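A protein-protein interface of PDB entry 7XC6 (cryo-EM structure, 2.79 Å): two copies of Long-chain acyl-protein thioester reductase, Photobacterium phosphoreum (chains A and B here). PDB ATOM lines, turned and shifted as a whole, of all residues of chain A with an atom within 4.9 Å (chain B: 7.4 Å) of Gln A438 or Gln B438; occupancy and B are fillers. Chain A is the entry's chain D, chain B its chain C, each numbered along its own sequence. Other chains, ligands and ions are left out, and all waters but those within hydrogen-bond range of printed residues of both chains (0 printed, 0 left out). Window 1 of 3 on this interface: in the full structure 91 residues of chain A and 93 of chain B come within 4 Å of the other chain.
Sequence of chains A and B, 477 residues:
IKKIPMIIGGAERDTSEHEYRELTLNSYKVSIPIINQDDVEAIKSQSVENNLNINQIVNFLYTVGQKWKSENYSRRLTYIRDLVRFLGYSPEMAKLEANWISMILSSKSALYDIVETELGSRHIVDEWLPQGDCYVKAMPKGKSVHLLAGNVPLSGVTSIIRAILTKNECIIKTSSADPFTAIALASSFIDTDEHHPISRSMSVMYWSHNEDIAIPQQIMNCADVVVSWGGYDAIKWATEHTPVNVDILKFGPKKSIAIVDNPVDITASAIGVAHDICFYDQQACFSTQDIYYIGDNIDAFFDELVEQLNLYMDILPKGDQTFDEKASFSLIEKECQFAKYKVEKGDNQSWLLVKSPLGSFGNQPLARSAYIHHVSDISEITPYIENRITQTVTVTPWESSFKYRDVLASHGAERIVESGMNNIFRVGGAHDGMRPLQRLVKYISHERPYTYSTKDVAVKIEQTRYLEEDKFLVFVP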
ATOM      1  N   GLU A 118     -31.351   0.061  14.682  1.00  0.00           N
ATOM      2  CA  GLU A 118     -30.965   1.404  14.274  1.00  0.00           C
ATOM      3  C   GLU A 118     -30.714   2.318  15.468  1.00  0.00           C
ATOM      4  O   GLU A 118     -29.752   3.091  15.459  1.00  0.00           O
ATOM      5  CB  GLU A 118     -32.023   1.991  13.351  1.00  0.00           C
ATOM      6  CG  GLU A 118     -32.210   1.188  12.082  1.00  0.00           C
ATOM      7  CD  GLU A 118     -32.837   1.992  10.969  1.00  0.00           C
ATOM      8  OE1 GLU A 118     -32.687   3.230  10.975  1.00  0.00           O
ATOM      9  OE2 GLU A 118     -33.473   1.390  10.082  1.00  0.00           O
ATOM     10  N   LEU A 119     -31.541   2.243  16.509  1.00  0.00           N
ATOM     11  CA  LEU A 119     -31.388   3.140  17.645  1.00  0.00           C
ATOM     12  C   LEU A 119     -30.660   2.513  18.822  1.00  0.00           C
ATOM     13  O   LEU A 119     -30.281   3.237  19.747  1.00  0.00           O
ATOM     14  CB  LEU A 119     -32.754   3.649  18.109  1.00  0.00           C
ATOM     15  CG  LEU A 119     -33.557   4.433  17.074  1.00  0.00           C
ATOM     16  CD1 LEU A 119     -34.882   4.872  17.643  1.00  0.00           C
ATOM     17  CD2 LEU A 119     -32.775   5.625  16.589  1.00  0.00           C
ATOM     18  N   ARG A 435     -28.784   4.418   8.162  1.00  0.00           N
ATOM     19  CA  ARG A 435     -29.855   3.858   8.970  1.00  0.00           C
ATOM     20  C   ARG A 435     -30.886   4.954   9.194  1.00  0.00           C
ATOM     21  O   ARG A 435     -30.664   5.863   9.999  1.00  0.00           O
ATOM     22  CB  ARG A 435     -29.309   3.296  10.279  1.00  0.00           C
ATOM     23  CG  ARG A 435     -28.768   1.897  10.107  1.00  0.00           C
ATOM     24  CD  ARG A 435     -27.997   1.414  11.302  1.00  0.00           C
ATOM     25  NE  ARG A 435     -27.807  -0.029  11.240  1.00  0.00           N
ATOM     26  CZ  ARG A 435     -27.010  -0.715  12.048  1.00  0.00           C
ATOM     27  NH1 ARG A 435     -26.318  -0.088  12.984  1.00  0.00           N
ATOM     28  NH2 ARG A 435     -26.906  -2.027  11.917  1.00  0.00           N
ATOM     29  N   PRO A 436     -32.023   4.895   8.497  1.00  0.00           N
ATOM     30  CA  PRO A 436     -32.828   6.112   8.317  1.00  0.00           C
ATOM     31  C   PRO A 436     -33.401   6.687   9.596  1.00  0.00           C
ATOM     32  O   PRO A 436     -33.351   7.908   9.778  1.00  0.00           O
ATOM     33  CB  PRO A 436     -33.930   5.651   7.356  1.00  0.00           C
ATOM     34  CG  PRO A 436     -33.344   4.483   6.657  1.00  0.00           C
ATOM     35  CD  PRO A 436     -32.540   3.780   7.692  1.00  0.00           C
ATOM     36  N   LEU A 437     -33.941   5.870  10.491  1.00  0.00           N
ATOM     37  CA  LEU A 437     -34.576   6.462  11.660  1.00  0.00           C
ATOM     38  C   LEU A 437     -33.584   6.832  12.750  1.00  0.00           C
ATOM     39  O   LEU A 437     -34.005   7.153  13.863  1.00  0.00           O
ATOM     40  CB  LEU A 437     -35.672   5.546  12.211  1.00  0.00           C
ATOM     41  CG  LEU A 437     -35.490   4.063  12.477  1.00  0.00           C
ATOM     42  CD1 LEU A 437     -34.971   3.856  13.866  1.00  0.00           C
ATOM     43  CD2 LEU A 437     -36.824   3.387  12.324  1.00  0.00           C
ATOM     44  N   GLN A 438     -32.285   6.798  12.460  1.00  0.00           N
ATOM     45  CA  GLN A 438     -31.335   7.531  13.287  1.00  0.00           C
ATOM     46  C   GLN A 438     -31.427   9.022  13.020  1.00  0.00           C
ATOM     47  O   GLN A 438     -31.073   9.831  13.882  1.00  0.00           O
ATOM     48  CB  GLN A 438     -29.915   7.047  13.029  1.00  0.00           C
ATOM     49  CG  GLN A 438     -29.589   5.718  13.646  1.00  0.00           C
ATOM     50  CD  GLN A 438     -28.233   5.222  13.226  1.00  0.00           C
ATOM     51  OE1 GLN A 438     -27.595   5.803  12.353  1.00  0.00           O
ATOM     52  NE2 GLN A 438     -27.780   4.144  13.843  1.00  0.00           N
ATOM     53  N   ARG A 439     -31.890   9.398  11.832  1.00  0.00           N
ATOM     54  CA  ARG A 439     -32.036  10.789  11.447  1.00  0.00           C
ATOM     55  C   ARG A 439     -33.456  11.306  11.607  1.00  0.00           C
ATOM     56  O   ARG A 439     -33.678  12.510  11.466  1.00  0.00           O
ATOM     57  CB  ARG A 439     -31.581  10.977  10.001  1.00  0.00           C
ATOM     58  CG  ARG A 439     -30.101  10.755   9.809  1.00  0.00           C
ATOM     59  CD  ARG A 439     -29.836   9.608   8.872  1.00  0.00           C
ATOM     60  NE  ARG A 439     -28.408   9.369   8.690  1.00  0.00           N
ATOM     61  CZ  ARG A 439     -27.614  10.126   7.943  1.00  0.00           C
ATOM     62  NH1 ARG A 439     -28.104  11.175   7.302  1.00  0.00           N
ATOM     63  NH2 ARG A 439     -26.329   9.831   7.833  1.00  0.00           N
ATOM     64  N   LEU A 440     -34.413  10.433  11.892  1.00  0.00           N
ATOM     65  CA  LEU A 440     -35.769  10.830  12.228  1.00  0.00           C
ATOM     66  C   LEU A 440     -35.950  11.032  13.722  1.00  0.00           C
ATOM     67  O   LEU A 440     -37.082  11.182  14.185  1.00  0.00           O
ATOM     68  CB  LEU A 440     -36.759   9.783  11.724  1.00  0.00           C
ATOM     69  CG  LEU A 440     -36.780   9.567  10.218  1.00  0.00           C
ATOM     70  CD1 LEU A 440     -37.461   8.263   9.894  1.00  0.00           C
ATOM     71  CD2 LEU A 440     -37.484  10.720   9.545  1.00  0.00           C
ATOM     72  N   VAL A 441     -34.862  11.051  14.476  1.00  0.00           N
ATOM     73  CA  VAL A 441     -34.893  11.031  15.928  1.00  0.00           C
ATOM     74  C   VAL A 441     -33.938  12.085  16.465  1.00  0.00           C
ATOM     75  O   VAL A 441     -32.898  12.375  15.869  1.00  0.00           O
ATOM     76  CB  VAL A 441     -34.544   9.621  16.459  1.00  0.00           C
ATOM     77  CG1 VAL A 441     -33.692   9.686  17.700  1.00  0.00           C
ATOM     78  CG2 VAL A 441     -35.812   8.861  16.756  1.00  0.00           C
ATOM     79  N   TYR A 443     -31.698  12.676  19.674  1.00  0.00           N
ATOM     80  CA  TYR A 443     -31.112  12.021  20.836  1.00  0.00           C
ATOM     81  C   TYR A 443     -30.964  13.050  21.945  1.00  0.00           C
ATOM     82  O   TYR A 443     -30.155  13.974  21.835  1.00  0.00           O
ATOM     83  CB  TYR A 443     -29.757  11.420  20.486  1.00  0.00           C
ATOM     84  CG  TYR A 443     -29.819  10.147  19.695  1.00  0.00           C
ATOM     85  CD1 TYR A 443     -30.163   8.952  20.297  1.00  0.00           C
ATOM     86  CD2 TYR A 443     -29.509  10.137  18.347  1.00  0.00           C
ATOM     87  CE1 TYR A 443     -30.209   7.786  19.577  1.00  0.00           C
ATOM     88  CE2 TYR A 443     -29.553   8.979  17.621  1.00  0.00           C
ATOM     89  CZ  TYR A 443     -29.901   7.807  18.240  1.00  0.00           C
ATOM     90  OH  TYR A 443     -29.940   6.647  17.512  1.00  0.00           O
ATOM     91  N   THR B 117     -21.038   3.777  21.662  1.00  0.00           N
ATOM     92  CA  THR B 117     -22.382   4.279  21.916  1.00  0.00           C
ATOM     93  C   THR B 117     -23.025   4.814  20.648  1.00  0.00           C
ATOM     94  O   THR B 117     -24.241   4.691  20.470  1.00  0.00           O
ATOM     95  CB  THR B 117     -22.352   5.357  22.995  1.00  0.00           C
ATOM     96  OG1 THR B 117     -21.398   6.363  22.641  1.00  0.00           O
ATOM     97  CG2 THR B 117     -21.979   4.755  24.336  1.00  0.00           C
ATOM     98  N   GLU B 118     -22.240   5.410  19.751  1.00  0.00           N
ATOM     99  CA  GLU B 118     -22.862   5.997  18.572  1.00  0.00           C
ATOM    100  C   GLU B 118     -23.099   4.968  17.474  1.00  0.00           C
ATOM    101  O   GLU B 118     -24.156   4.978  16.838  1.00  0.00           O
ATOM    102  CB  GLU B 118     -22.017   7.157  18.061  1.00  0.00           C
ATOM    103  CG  GLU B 118     -21.869   8.270  19.075  1.00  0.00           C
ATOM    104  CD  GLU B 118     -21.503   9.590  18.442  1.00  0.00           C
ATOM    105  OE1 GLU B 118     -21.830   9.789  17.256  1.00  0.00           O
ATOM    106  OE2 GLU B 118     -20.896  10.435  19.130  1.00  0.00           O
ATOM    107  N   LEU B 119     -22.151   4.061  17.240  1.00  0.00           N
ATOM    108  CA  LEU B 119     -22.296   3.100  16.157  1.00  0.00           C
ATOM    109  C   LEU B 119     -22.780   1.734  16.617  1.00  0.00           C
ATOM    110  O   LEU B 119     -23.147   0.913  15.773  1.00  0.00           O
ATOM    111  CB  LEU B 119     -20.972   2.939  15.407  1.00  0.00           C
ATOM    112  CG  LEU B 119     -20.422   4.206  14.756  1.00  0.00           C
ATOM    113  CD1 LEU B 119     -19.116   3.924  14.057  1.00  0.00           C
ATOM    114  CD2 LEU B 119     -21.420   4.782  13.788  1.00  0.00           C
ATOM    115  N   GLY B 120     -22.795   1.467  17.923  1.00  0.00           N
ATOM    116  CA  GLY B 120     -23.245   0.207  18.469  1.00  0.00           C
ATOM    117  C   GLY B 120     -22.118  -0.685  18.943  1.00  0.00           C
ATOM    118  O   GLY B 120     -22.301  -1.445  19.901  1.00  0.00           O
ATOM    119  N   LYS B 141     -16.920   7.790   4.923  1.00  0.00           N
ATOM    120  CA  LYS B 141     -17.405   8.500   3.746  1.00  0.00           C
ATOM    121  C   LYS B 141     -16.250   9.014   2.900  1.00  0.00           C
ATOM    122  O   LYS B 141     -16.327   9.004   1.668  1.00  0.00           O
ATOM    123  CB  LYS B 141     -18.316   9.651   4.159  1.00  0.00           C
ATOM    124  CG  LYS B 141     -19.509   9.225   4.972  1.00  0.00           C
ATOM    125  CD  LYS B 141     -20.767   9.893   4.472  1.00  0.00           C
ATOM    126  CE  LYS B 141     -21.994   9.278   5.099  1.00  0.00           C
ATOM    127  NZ  LYS B 141     -23.174  10.167   4.970  1.00  0.00           N
ATOM    128  N   THR B 166     -13.636   7.582  12.486  1.00  0.00           N
ATOM    129  CA  THR B 166     -14.373   6.894  11.441  1.00  0.00           C
ATOM    130  C   THR B 166     -13.542   6.694  10.184  1.00  0.00           C
ATOM    131  O   THR B 166     -14.091   6.307   9.149  1.00  0.00           O
ATOM    132  CB  THR B 166     -15.654   7.658  11.112  1.00  0.00           C
ATOM    133  OG1 THR B 166     -15.339   9.030  10.858  1.00  0.00           O
ATOM    134  CG2 THR B 166     -16.617   7.586  12.275  1.00  0.00           C
ATOM    135  N   ASP B 247     -24.289  14.811   2.365  1.00  0.00           N
ATOM    136  CA  ASP B 247     -24.906  15.113   3.646  1.00  0.00           C
ATOM    137  C   ASP B 247     -24.133  16.199   4.380  1.00  0.00           C
ATOM    138  O   ASP B 247     -22.917  16.332   4.233  1.00  0.00           O
ATOM    139  CB  ASP B 247     -24.976  13.859   4.515  1.00  0.00           C
ATOM    140  CG  ASP B 247     -25.959  13.997   5.653  1.00  0.00           C
ATOM    141  OD1 ASP B 247     -25.806  13.277   6.662  1.00  0.00           O
ATOM    142  OD2 ASP B 247     -26.892  14.819   5.537  1.00  0.00           O
ATOM    143  N   LEU B 249     -23.650  17.876   8.267  1.00  0.00           N
ATOM    144  CA  LEU B 249     -23.857  17.921   9.710  1.00  0.00           C
ATOM    145  C   LEU B 249     -23.885  19.383  10.130  1.00  0.00           C
ATOM    146  O   LEU B 249     -22.865  20.073  10.058  1.00  0.00           O
ATOM    147  CB  LEU B 249     -22.754  17.164  10.443  1.00  0.00           C
ATOM    148  CG  LEU B 249     -22.844  15.645  10.507  1.00  0.00           C
ATOM    149  CD1 LEU B 249     -22.296  15.039   9.235  1.00  0.00           C
ATOM    150  CD2 LEU B 249     -22.082  15.133  11.706  1.00  0.00           C
ATOM    151  N   GLY B 433     -28.824  17.020  19.723  1.00  0.00           N
ATOM    152  CA  GLY B 433     -29.806  16.002  19.409  1.00  0.00           C
ATOM    153  C   GLY B 433     -29.372  15.070  18.307  1.00  0.00           C
ATOM    154  O   GLY B 433     -30.214  14.521  17.595  1.00  0.00           O
ATOM    155  N   MET B 434     -28.070  14.874  18.152  1.00  0.00           N
ATOM    156  CA  MET B 434     -27.519  14.176  17.003  1.00  0.00           C
ATOM    157  C   MET B 434     -26.258  13.457  17.440  1.00  0.00           C
ATOM    158  O   MET B 434     -25.391  14.062  18.073  1.00  0.00           O
ATOM    159  CB  MET B 434     -27.218  15.164  15.874  1.00  0.00           C
ATOM    160  CG  MET B 434     -26.143  14.727  14.913  1.00  0.00           C
ATOM    161  SD  MET B 434     -26.100  15.776  13.452  1.00  0.00           S
ATOM    162  CE  MET B 434     -25.648  17.345  14.175  1.00  0.00           C
ATOM    163  N   ARG B 435     -26.170  12.175  17.129  1.00  0.00           N
ATOM    164  CA  ARG B 435     -24.940  11.443  17.385  1.00  0.00           C
ATOM    165  C   ARG B 435     -24.061  11.575  16.151  1.00  0.00           C
ATOM    166  O   ARG B 435     -24.314  10.926  15.131  1.00  0.00           O
ATOM    167  CB  ARG B 435     -25.239   9.989  17.732  1.00  0.00           C
ATOM    168  CG  ARG B 435     -25.589   9.821  19.192  1.00  0.00           C
ATOM    169  CD  ARG B 435     -26.133   8.457  19.514  1.00  0.00           C
ATOM    170  NE  ARG B 435     -26.117   8.227  20.952  1.00  0.00           N
ATOM    171  CZ  ARG B 435     -26.705   7.200  21.552  1.00  0.00           C
ATOM    172  NH1 ARG B 435     -27.364   6.304  20.836  1.00  0.00           N
ATOM    173  NH2 ARG B 435     -26.633   7.071  22.865  1.00  0.00           N
ATOM    174  N   PRO B 436     -23.017  12.407  16.213  1.00  0.00           N
ATOM    175  CA  PRO B 436     -22.426  12.922  14.969  1.00  0.00           C
ATOM    176  C   PRO B 436     -21.793  11.867  14.086  1.00  0.00           C
ATOM    177  O   PRO B 436     -21.997  11.906  12.867  1.00  0.00           O
ATOM    178  CB  PRO B 436     -21.390  13.931  15.480  1.00  0.00           C
ATOM    179  CG  PRO B 436     -21.881  14.312  16.826  1.00  0.00           C
ATOM    180  CD  PRO B 436     -22.444  13.061  17.397  1.00  0.00           C
ATOM    181  N   LEU B 437     -21.037  10.925  14.636  1.00  0.00           N
ATOM    182  CA  LEU B 437     -20.361   9.989  13.750  1.00  0.00           C
ATOM    183  C   LEU B 437     -21.258   8.853  13.290  1.00  0.00           C
ATOM    184  O   LEU B 437     -20.759   7.891  12.703  1.00  0.00           O
ATOM    185  CB  LEU B 437     -19.085   9.445  14.399  1.00  0.00           C
ATOM    186  CG  LEU B 437     -19.016   8.888  15.810  1.00  0.00           C
ATOM    187  CD1 LEU B 437     -19.330   7.425  15.794  1.00  0.00           C
ATOM    188  CD2 LEU B 437     -17.626   9.106  16.339  1.00  0.00           C
ATOM    189  N   GLN B 438     -22.564   8.940  13.536  1.00  0.00           N
ATOM    190  CA  GLN B 438     -23.502   8.133  12.770  1.00  0.00           C
ATOM    191  C   GLN B 438     -23.662   8.679  11.363  1.00  0.00           C
ATOM    192  O   GLN B 438     -24.024   7.938  10.445  1.00  0.00           O
ATOM    193  CB  GLN B 438     -24.859   8.089  13.461  1.00  0.00           C
ATOM    194  CG  GLN B 438     -24.913   7.198  14.668  1.00  0.00           C
ATOM    195  CD  GLN B 438     -26.224   7.319  15.396  1.00  0.00           C
ATOM    196  OE1 GLN B 438     -27.039   8.182  15.083  1.00  0.00           O
ATOM    197  NE2 GLN B 438     -26.438   6.455  16.375  1.00  0.00           N
ATOM    198  N   ARG B 439     -23.403   9.970  11.180  1.00  0.00           N
ATOM    199  CA  ARG B 439     -23.506  10.621   9.887  1.00  0.00           C
ATOM    200  C   ARG B 439     -22.168  10.765   9.184  1.00  0.00           C
ATOM    201  O   ARG B 439     -22.142  11.155   8.015  1.00  0.00           O
ATOM    202  CB  ARG B 439     -24.153  11.994  10.050  1.00  0.00           C
ATOM    203  CG  ARG B 439     -25.597  11.925  10.481  1.00  0.00           C
ATOM    204  CD  ARG B 439     -25.804  12.588  11.816  1.00  0.00           C
ATOM    205  NE  ARG B 439     -27.193  12.514  12.254  1.00  0.00           N
ATOM    206  CZ  ARG B 439     -28.173  13.264  11.763  1.00  0.00           C
ATOM    207  NH1 ARG B 439     -27.920  14.150  10.813  1.00  0.00           N
ATOM    208  NH2 ARG B 439     -29.404  13.131  12.225  1.00  0.00           N
ATOM    209  N   LEU B 440     -21.068  10.467   9.862  1.00  0.00           N
ATOM    210  CA  LEU B 440     -19.754  10.409   9.247  1.00  0.00           C
ATOM    211  C   LEU B 440     -19.426   9.021   8.728  1.00  0.00           C
ATOM    212  O   LEU B 440     -18.281   8.762   8.355  1.00  0.00           O
ATOM    213  CB  LEU B 440     -18.688  10.851  10.249  1.00  0.00           C
ATOM    214  CG  LEU B 440     -18.816  12.280  10.757  1.00  0.00           C
ATOM    215  CD1 LEU B 440     -17.997  12.455  12.009  1.00  0.00           C
ATOM    216  CD2 LEU B 440     -18.373  13.248   9.689  1.00  0.00           C
ATOM    217  N   VAL B 441     -20.409   8.133   8.689  1.00  0.00           N
ATOM    218  CA  VAL B 441     -20.202   6.722   8.412  1.00  0.00           C
ATOM    219  C   VAL B 441     -21.228   6.254   7.393  1.00  0.00           C
ATOM    220  O   VAL B 441     -22.363   6.736   7.355  1.00  0.00           O
ATOM    221  CB  VAL B 441     -20.276   5.896   9.718  1.00  0.00           C
ATOM    222  CG1 VAL B 441     -20.975   4.579   9.507  1.00  0.00           C
ATOM    223  CG2 VAL B 441     -18.885   5.652  10.246  1.00  0.00           C
ATOM    224  N   LYS B 442     -20.806   5.324   6.546  1.00  0.00           N
ATOM    225  CA  LYS B 442     -21.658   4.646   5.582  1.00  0.00           C
ATOM    226  C   LYS B 442     -21.889   3.236   6.103  1.00  0.00           C
ATOM    227  O   LYS B 442     -20.942   2.454   6.225  1.00  0.00           O
ATOM    228  CB  LYS B 442     -20.989   4.629   4.213  1.00  0.00           C
ATOM    229  CG  LYS B 442     -21.923   4.587   3.040  1.00  0.00           C
ATOM    230  CD  LYS B 442     -21.164   4.171   1.799  1.00  0.00           C
ATOM    231  CE  LYS B 442     -20.000   5.109   1.538  1.00  0.00           C
ATOM    232  NZ  LYS B 442     -19.197   4.674   0.367  1.00  0.00           N
ATOM    233  N   TYR B 443     -23.131   2.918   6.440  1.00  0.00           N
ATOM    234  CA  TYR B 443     -23.474   1.583   6.913  1.00  0.00           C
ATOM    235  C   TYR B 443     -23.636   0.672   5.708  1.00  0.00           C
ATOM    236  O   TYR B 443     -24.577   0.830   4.928  1.00  0.00           O
ATOM    237  CB  TYR B 443     -24.758   1.616   7.730  1.00  0.00           C
ATOM    238  CG  TYR B 443     -24.608   2.162   9.118  1.00  0.00           C
ATOM    239  CD1 TYR B 443     -24.025   1.407  10.118  1.00  0.00           C
ATOM    240  CD2 TYR B 443     -25.071   3.425   9.436  1.00  0.00           C
ATOM    241  CE1 TYR B 443     -23.898   1.900  11.391  1.00  0.00           C
ATOM    242  CE2 TYR B 443     -24.947   3.926  10.703  1.00  0.00           C
ATOM    243  CZ  TYR B 443     -24.362   3.160  11.677  1.00  0.00           C
ATOM    244  OH  TYR B 443     -24.242   3.661  12.946  1.00  0.00           O
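Among the printed residues, merely in contact across the chains: Tyr A443 with Arg B435, Arg A439 with Arg B439, Arg A435 with Tyr B443, Gln A438 with Gln B438, Gln A438 with Tyr B443, Tyr A443 with Gln B438, Val A441 with Gly B433 and Arg A439 with Gln B438.
Arg A435 touches Tyr B443, and with the chains exchanged Tyr A443 touches Arg B435. Gln A438 touches its own counterpart, Gln B438. Gln A438 touches Tyr B443, and with the chains exchanged Tyr A443 touches Gln B438. Arg B439 touches its own counterpart, Arg A439.
Gln A438 touches just these residues of chain B: Gln B438 (3.6 Å) and Tyr B443 (3.6 Å). Of chain A, only Gln A438 (3.6 Å), Arg A439 (3.96 Å) and Tyr A443 (3.7 Å) come within 4 Å of Gln B438. Printed residues of chain B within 4 Å of Arg A439: Asp B247, Gln B438 and Arg B439. Of the printed residues of chain B, Arg A435 touches Tyr B443. The nearest residue of chain A that does not touch Gln B438 is Glu A118 (4.8 Å).
O of Glu B118 lies within hydrogen-bond range of NE2 of Gln B438, at 2.8 Å. The backbone carbonyl oxygen of Arg B439 sits at hydrogen-bond distance from the side-chain amino group of Lys B141 (3.4 Å). NH1 of Arg B439 lies within hydrogen-bond range of SD of Met B434 (3.6 Å). NE2 of Gln A438 sits at hydrogen-bond distance from O of Glu A118 (2.8 Å).
Of the 19 printed residues of chain B, 6 touch a printed residue of chain A. Among the printed residues, Asp or Glu carboxylates within 4 Å of a Lys or Arg side-chain nitrogen of the other chain: Arg A439 with Asp B247 (3.2 Å).
The side-chain carboxylate (OD1) of Asp B247 lies within salt-bridge range of the guanidinium group (NH1) of Arg A439. The backbone NH (N) of Tyr A443 sits at hydrogen-bond distance from the backbone carbonyl oxygen (O) of Gly B433 (3.2 Å).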
